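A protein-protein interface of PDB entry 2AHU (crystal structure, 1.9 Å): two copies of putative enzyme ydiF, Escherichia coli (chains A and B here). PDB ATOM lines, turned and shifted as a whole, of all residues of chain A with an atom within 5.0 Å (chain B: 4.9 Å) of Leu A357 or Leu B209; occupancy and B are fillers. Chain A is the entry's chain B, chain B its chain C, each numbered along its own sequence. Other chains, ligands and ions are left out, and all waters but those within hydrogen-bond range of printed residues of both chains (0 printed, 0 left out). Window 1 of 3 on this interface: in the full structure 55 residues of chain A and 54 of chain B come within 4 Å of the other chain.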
ATOM      1  N   TYR A 205       9.583 -26.644  -2.170  1.00  0.00           N
ATOM      2  CA  TYR A 205       8.931 -25.432  -1.670  1.00  0.00           C
ATOM      3  C   TYR A 205       7.865 -24.905  -2.607  1.00  0.00           C
ATOM      4  O   TYR A 205       6.949 -24.200  -2.169  1.00  0.00           O
ATOM      5  CB  TYR A 205       9.946 -24.314  -1.466  1.00  0.00           C
ATOM      6  CG  TYR A 205      11.141 -24.644  -0.621  1.00  0.00           C
ATOM      7  CD1 TYR A 205      11.002 -25.178   0.665  1.00  0.00           C
ATOM      8  CD2 TYR A 205      12.421 -24.376  -1.092  1.00  0.00           C
ATOM      9  CE1 TYR A 205      12.128 -25.461   1.446  1.00  0.00           C
ATOM     10  CE2 TYR A 205      13.538 -24.646  -0.327  1.00  0.00           C
ATOM     11  CZ  TYR A 205      13.392 -25.183   0.936  1.00  0.00           C
ATOM     12  OH  TYR A 205      14.524 -25.437   1.681  1.00  0.00           O
ATOM     13  N   THR A 334      10.388 -27.316 -10.732  1.00  0.00           N
ATOM     14  CA  THR A 334       9.698 -27.066  -9.461  1.00  0.00           C
ATOM     15  C   THR A 334      10.638 -26.680  -8.321  1.00  0.00           C
ATOM     16  O   THR A 334      10.174 -26.329  -7.224  1.00  0.00           O
ATOM     17  CB  THR A 334       8.850 -28.289  -9.031  1.00  0.00           C
ATOM     18  OG1 THR A 334       9.626 -29.487  -9.152  1.00  0.00           O
ATOM     19  CG2 THR A 334       7.665 -28.513  -9.963  1.00  0.00           C
ATOM     20  N   GLY A 335      11.949 -26.759  -8.563  1.00  0.00           N
ATOM     21  CA  GLY A 335      12.915 -26.348  -7.554  1.00  0.00           C
ATOM     22  C   GLY A 335      14.137 -27.218  -7.274  1.00  0.00           C
ATOM     23  O   GLY A 335      15.232 -26.672  -7.139  1.00  0.00           O
ATOM     24  N   PRO A 336      13.980 -28.541  -7.152  1.00  0.00           N
ATOM     25  CA  PRO A 336      15.118 -29.402  -6.807  1.00  0.00           C
ATOM     26  C   PRO A 336      16.228 -29.411  -7.866  1.00  0.00           C
ATOM     27  O   PRO A 336      15.953 -29.420  -9.075  1.00  0.00           O
ATOM     28  CB  PRO A 336      14.489 -30.795  -6.672  1.00  0.00           C
ATOM     29  CG  PRO A 336      13.032 -30.544  -6.478  1.00  0.00           C
ATOM     30  CD  PRO A 336      12.735 -29.320  -7.287  1.00  0.00           C
ATOM     31  N   ILE A 337      17.465 -29.418  -7.388  1.00  0.00           N
ATOM     32  CA  ILE A 337      18.645 -29.409  -8.236  1.00  0.00           C
ATOM     33  C   ILE A 337      19.480 -30.659  -7.965  1.00  0.00           C
ATOM     34  O   ILE A 337      19.912 -30.897  -6.835  1.00  0.00           O
ATOM     35  CB  ILE A 337      19.468 -28.119  -8.001  1.00  0.00           C
ATOM     36  CG1 ILE A 337      18.658 -26.895  -8.456  1.00  0.00           C
ATOM     37  CG2 ILE A 337      20.803 -28.176  -8.762  1.00  0.00           C
ATOM     38  CD1 ILE A 337      19.116 -25.597  -7.855  1.00  0.00           C
ATOM     39  N   ALA A 355      20.555 -28.911  -4.015  1.00  0.00           N
ATOM     40  CA  ALA A 355      19.927 -27.653  -3.632  1.00  0.00           C
ATOM     41  C   ALA A 355      18.460 -27.730  -4.000  1.00  0.00           C
ATOM     42  O   ALA A 355      18.059 -28.544  -4.854  1.00  0.00           O
ATOM     43  CB  ALA A 355      20.595 -26.460  -4.363  1.00  0.00           C
ATOM     44  N   ILE A 356      17.659 -26.899  -3.341  1.00  0.00           N
ATOM     45  CA  ILE A 356      16.248 -26.735  -3.676  1.00  0.00           C
ATOM     46  C   ILE A 356      15.949 -25.240  -3.677  1.00  0.00           C
ATOM     47  O   ILE A 356      16.035 -24.598  -2.633  1.00  0.00           O
ATOM     48  CB  ILE A 356      15.329 -27.471  -2.659  1.00  0.00           C
ATOM     49  CG1 ILE A 356      15.751 -28.938  -2.518  1.00  0.00           C
ATOM     50  CG2 ILE A 356      13.863 -27.327  -3.087  1.00  0.00           C
ATOM     51  CD1 ILE A 356      14.876 -29.805  -1.637  1.00  0.00           C
ATOM     52  N   LEU A 357      15.635 -24.694  -4.849  1.00  0.00           N
ATOM     53  CA  LEU A 357      15.216 -23.298  -4.963  1.00  0.00           C
ATOM     54  C   LEU A 357      13.699 -23.233  -4.943  1.00  0.00           C
ATOM     55  O   LEU A 357      13.041 -24.232  -5.215  1.00  0.00           O
ATOM     56  CB  LEU A 357      15.691 -22.686  -6.281  1.00  0.00           C
ATOM     57  CG  LEU A 357      17.159 -22.550  -6.662  1.00  0.00           C
ATOM     58  CD1 LEU A 357      17.217 -21.941  -8.064  1.00  0.00           C
ATOM     59  CD2 LEU A 357      17.939 -21.711  -5.661  1.00  0.00           C
ATOM     60  N   ASP A 358      13.141 -22.057  -4.644  1.00  0.00           N
ATOM     61  CA  ASP A 358      11.715 -21.850  -4.867  1.00  0.00           C
ATOM     62  C   ASP A 358      11.444 -21.893  -6.374  1.00  0.00           C
ATOM     63  O   ASP A 358      12.317 -21.555  -7.191  1.00  0.00           O
ATOM     64  CB  ASP A 358      11.201 -20.544  -4.242  1.00  0.00           C
ATOM     65  CG  ASP A 358      11.721 -19.313  -4.945  1.00  0.00           C
ATOM     66  OD1 ASP A 358      10.974 -18.713  -5.756  1.00  0.00           O
ATOM     67  OD2 ASP A 358      12.878 -18.873  -4.754  1.00  0.00           O
ATOM     68  N   MET A 359      10.236 -22.317  -6.732  1.00  0.00           N
ATOM     69  CA  MET A 359       9.890 -22.542  -8.124  1.00  0.00           C
ATOM     70  C   MET A 359       9.976 -21.287  -8.994  1.00  0.00           C
ATOM     71  O   MET A 359      10.431 -21.364 -10.131  1.00  0.00           O
ATOM     72  CB  MET A 359       8.498 -23.161  -8.235  1.00  0.00           C
ATOM     73  CG  MET A 359       8.087 -23.477  -9.658  1.00  0.00           C
ATOM     74  SD  MET A 359       6.430 -24.457  -9.765  1.00  0.00           S
ATOM     75  CE  MET A 359       5.276 -23.174  -8.917  1.00  0.00           C
ATOM     76  N   SER A 361      11.877 -18.586  -8.753  1.00  0.00           N
ATOM     77  CA  SER A 361      13.301 -18.346  -9.000  1.00  0.00           C
ATOM     78  C   SER A 361      13.902 -19.280 -10.051  1.00  0.00           C
ATOM     79  O   SER A 361      14.721 -18.858 -10.863  1.00  0.00           O
ATOM     80  CB  SER A 361      14.093 -18.479  -7.696  1.00  0.00           C
ATOM     81  OG  SER A 361      13.627 -17.561  -6.728  1.00  0.00           O
ATOM     82  N   GLN A 362      13.494 -20.547 -10.028  1.00  0.00           N
ATOM     83  CA  GLN A 362      13.921 -21.530 -11.029  1.00  0.00           C
ATOM     84  C   GLN A 362      13.485 -21.142 -12.444  1.00  0.00           C
ATOM     85  O   GLN A 362      14.266 -21.220 -13.397  1.00  0.00           O
ATOM     86  CB  GLN A 362      13.365 -22.912 -10.675  1.00  0.00           C
ATOM     87  CG  GLN A 362      13.937 -24.053 -11.504  1.00  0.00           C
ATOM     88  CD  GLN A 362      15.343 -24.430 -11.089  1.00  0.00           C
ATOM     89  OE1 GLN A 362      16.269 -23.623 -11.197  1.00  0.00           O
ATOM     90  NE2 GLN A 362      15.508 -25.657 -10.614  1.00  0.00           N
ATOM     91  N   ASP B 207      19.819  -9.918  -1.874  1.00  0.00           N
ATOM     92  CA  ASP B 207      19.437 -10.427  -3.194  1.00  0.00           C
ATOM     93  C   ASP B 207      20.580 -11.144  -3.934  1.00  0.00           C
ATOM     94  O   ASP B 207      20.698 -11.046  -5.161  1.00  0.00           O
ATOM     95  CB  ASP B 207      18.864  -9.296  -4.060  1.00  0.00           C
ATOM     96  CG  ASP B 207      19.768  -8.069  -4.117  1.00  0.00           C
ATOM     97  OD1 ASP B 207      19.417  -7.121  -4.857  1.00  0.00           O
ATOM     98  OD2 ASP B 207      20.823  -7.938  -3.448  1.00  0.00           O
ATOM     99  N   ALA B 208      21.393 -11.883  -3.188  1.00  0.00           N
ATOM    100  CA  ALA B 208      22.561 -12.582  -3.737  1.00  0.00           C
ATOM    101  C   ALA B 208      22.236 -13.519  -4.900  1.00  0.00           C
ATOM    102  O   ALA B 208      22.922 -13.483  -5.930  1.00  0.00           O
ATOM    103  CB  ALA B 208      23.316 -13.333  -2.621  1.00  0.00           C
ATOM    104  N   LEU B 209      21.205 -14.356  -4.740  1.00  0.00           N
ATOM    105  CA  LEU B 209      20.775 -15.283  -5.798  1.00  0.00           C
ATOM    106  C   LEU B 209      20.325 -14.553  -7.075  1.00  0.00           C
ATOM    107  O   LEU B 209      20.756 -14.881  -8.180  1.00  0.00           O
ATOM    108  CB  LEU B 209      19.665 -16.224  -5.300  1.00  0.00           C
ATOM    109  CG  LEU B 209      19.080 -17.194  -6.346  1.00  0.00           C
ATOM    110  CD1 LEU B 209      20.125 -18.170  -6.895  1.00  0.00           C
ATOM    111  CD2 LEU B 209      17.876 -17.948  -5.805  1.00  0.00           C
ATOM    112  N   VAL B 210      19.464 -13.557  -6.905  1.00  0.00           N
ATOM    113  CA  VAL B 210      18.994 -12.727  -8.013  1.00  0.00           C
ATOM    114  C   VAL B 210      20.180 -12.099  -8.761  1.00  0.00           C
ATOM    115  O   VAL B 210      20.222 -12.134  -9.994  1.00  0.00           O
ATOM    116  CB  VAL B 210      18.040 -11.611  -7.506  1.00  0.00           C
ATOM    117  CG1 VAL B 210      17.918 -10.472  -8.526  1.00  0.00           C
ATOM    118  CG2 VAL B 210      16.652 -12.185  -7.165  1.00  0.00           C
ATOM    119  N   ILE B 211      21.132 -11.531  -8.020  1.00  0.00           N
ATOM    120  CA  ILE B 211      22.330 -10.938  -8.646  1.00  0.00           C
ATOM    121  C   ILE B 211      23.110 -11.982  -9.452  1.00  0.00           C
ATOM    122  O   ILE B 211      23.497 -11.722 -10.596  1.00  0.00           O
ATOM    123  CB  ILE B 211      23.239 -10.231  -7.613  1.00  0.00           C
ATOM    124  CG1 ILE B 211      22.552  -8.980  -7.049  1.00  0.00           C
ATOM    125  CG2 ILE B 211      24.589  -9.836  -8.264  1.00  0.00           C
ATOM    126  CD1 ILE B 211      23.246  -8.380  -5.818  1.00  0.00           C
ATOM    127  N   ALA B 212      23.335 -13.158  -8.861  1.00  0.00           N
ATOM    128  CA  ALA B 212      24.036 -14.238  -9.554  1.00  0.00           C
ATOM    129  C   ALA B 212      23.309 -14.699 -10.817  1.00  0.00           C
ATOM    130  O   ALA B 212      23.952 -14.948 -11.844  1.00  0.00           O
ATOM    131  CB  ALA B 212      24.272 -15.412  -8.626  1.00  0.00           C
ATOM    132  N   GLN B 213      21.983 -14.831 -10.749  1.00  0.00           N
ATOM    133  CA  GLN B 213      21.213 -15.226 -11.932  1.00  0.00           C
ATOM    134  C   GLN B 213      21.273 -14.169 -13.039  1.00  0.00           C
ATOM    135  O   GLN B 213      21.441 -14.510 -14.204  1.00  0.00           O
ATOM    136  CB  GLN B 213      19.760 -15.553 -11.590  1.00  0.00           C
ATOM    137  CG  GLN B 213      19.565 -16.807 -10.727  1.00  0.00           C
ATOM    138  CD  GLN B 213      18.100 -17.057 -10.418  1.00  0.00           C
ATOM    139  OE1 GLN B 213      17.309 -16.119 -10.371  1.00  0.00           O
ATOM    140  NE2 GLN B 213      17.740 -18.309 -10.213  1.00  0.00           N
ATOM    141  N   ARG B 241      21.710 -21.764  -0.808  1.00  0.00           N
ATOM    142  CA  ARG B 241      20.971 -20.631  -1.371  1.00  0.00           C
ATOM    143  C   ARG B 241      21.411 -20.289  -2.788  1.00  0.00           C
ATOM    144  O   ARG B 241      20.633 -19.733  -3.562  1.00  0.00           O
ATOM    145  CB  ARG B 241      21.116 -19.384  -0.488  1.00  0.00           C
ATOM    146  CG  ARG B 241      20.700 -19.574   0.979  1.00  0.00           C
ATOM    147  CD  ARG B 241      19.217 -19.783   1.184  1.00  0.00           C
ATOM    148  NE  ARG B 241      18.449 -18.591   0.805  1.00  0.00           N
ATOM    149  CZ  ARG B 241      17.228 -18.315   1.238  1.00  0.00           C
ATOM    150  NH1 ARG B 241      16.613 -19.138   2.077  1.00  0.00           N
ATOM    151  NH2 ARG B 241      16.616 -17.207   0.831  1.00  0.00           N
ATOM    152  N   ILE B 242      22.663 -20.601  -3.118  1.00  0.00           N
ATOM    153  CA  ILE B 242      23.172 -20.390  -4.472  1.00  0.00           C
ATOM    154  C   ILE B 242      23.719 -21.711  -5.033  1.00  0.00           C
ATOM    155  O   ILE B 242      24.635 -22.302  -4.458  1.00  0.00           O
ATOM    156  CB  ILE B 242      24.239 -19.270  -4.508  1.00  0.00           C
ATOM    157  CG1 ILE B 242      23.658 -17.956  -3.968  1.00  0.00           C
ATOM    158  CG2 ILE B 242      24.737 -19.048  -5.944  1.00  0.00           C
ATOM    159  CD1 ILE B 242      24.690 -16.898  -3.693  1.00  0.00           C
ATOM    160  N   PRO B 243      23.136 -22.188  -6.128  1.00  0.00           N
ATOM    161  CA  PRO B 243      23.649 -23.385  -6.795  1.00  0.00           C
ATOM    162  C   PRO B 243      24.986 -23.096  -7.464  1.00  0.00           C
ATOM    163  O   PRO B 243      25.197 -22.002  -7.998  1.00  0.00           O
ATOM    164  CB  PRO B 243      22.573 -23.714  -7.829  1.00  0.00           C
ATOM    165  CG  PRO B 243      21.803 -22.443  -8.032  1.00  0.00           C
ATOM    166  CD  PRO B 243      21.940 -21.635  -6.792  1.00  0.00           C
ATOM    167  N   LEU B 246      26.094 -21.321 -10.967  1.00  0.00           N
ATOM    168  CA  LEU B 246      25.969 -19.872 -11.130  1.00  0.00           C
ATOM    169  C   LEU B 246      27.262 -19.138 -10.815  1.00  0.00           C
ATOM    170  O   LEU B 246      27.379 -17.949 -11.107  1.00  0.00           O
ATOM    171  CB  LEU B 246      24.853 -19.319 -10.242  1.00  0.00           C
ATOM    172  CG  LEU B 246      23.423 -19.711 -10.610  1.00  0.00           C
ATOM    173  CD1 LEU B 246      22.476 -19.041  -9.642  1.00  0.00           C
ATOM    174  CD2 LEU B 246      23.115 -19.288 -12.055  1.00  0.00           C
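O of Ser A361 lies within hydrogen-bond range of NE2 of Gln B213, 3.1 Å away.
The backbone carbonyl oxygen (O) of Gly A335 sits at hydrogen-bond distance from the backbone NH (N) of Leu A357 (3.1 Å).
The backbone carbonyl oxygen (O) of Ala A355 lies within hydrogen-bond range of the backbone NH (N) of Ile A337, at 2.7 Å.
The side-chain carboxylate of Asp A358 lies within hydrogen-bond range of the side-chain hydroxyl of Ser A361, at 2.5 Å.
Among the printed residues, pairs that only touch across the chains: Leu A357 with Leu B209 (3.8 Å), Ile A337 with Pro B243 (3.9 Å) and Leu A357 with Arg B241 (3.9 Å).
Printed residues of chain B within 4 Å of Ile A337: Pro B243.
Ile A356 touches none of the printed residues of chain B.
Leu A357 touches two residues of chain B.
Of chain A, only Leu A357 (3.8 Å) comes within 4 Å of Leu B209.
Of the printed residues of chain A, Pro B243 touches Ile A337 (3.9 Å).
The nearest residue of chain B that does not touch Leu A357 is Pro B243 (4.2 Å).
The nearest residue of chain A that does not touch Leu B209 is Ser A361 (4.3 Å).
Of the 11 printed residues of chain B, 4 touch a printed residue of chain A.
Printed residues of chain B that touch a printed residue of chain A: Leu B209, Gln B213, Arg B241 and Pro B243.
Along chain A the printed residues that touch a printed residue of chain B span positions 337 to 361.
Among the printed residues, 4 pairs touch across the chains.
Among the printed residues, no Asp or Glu carboxylate lies within 4 Å of a Lys or Arg side-chain nitrogen of the other chain.
No position is printed for both chains.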
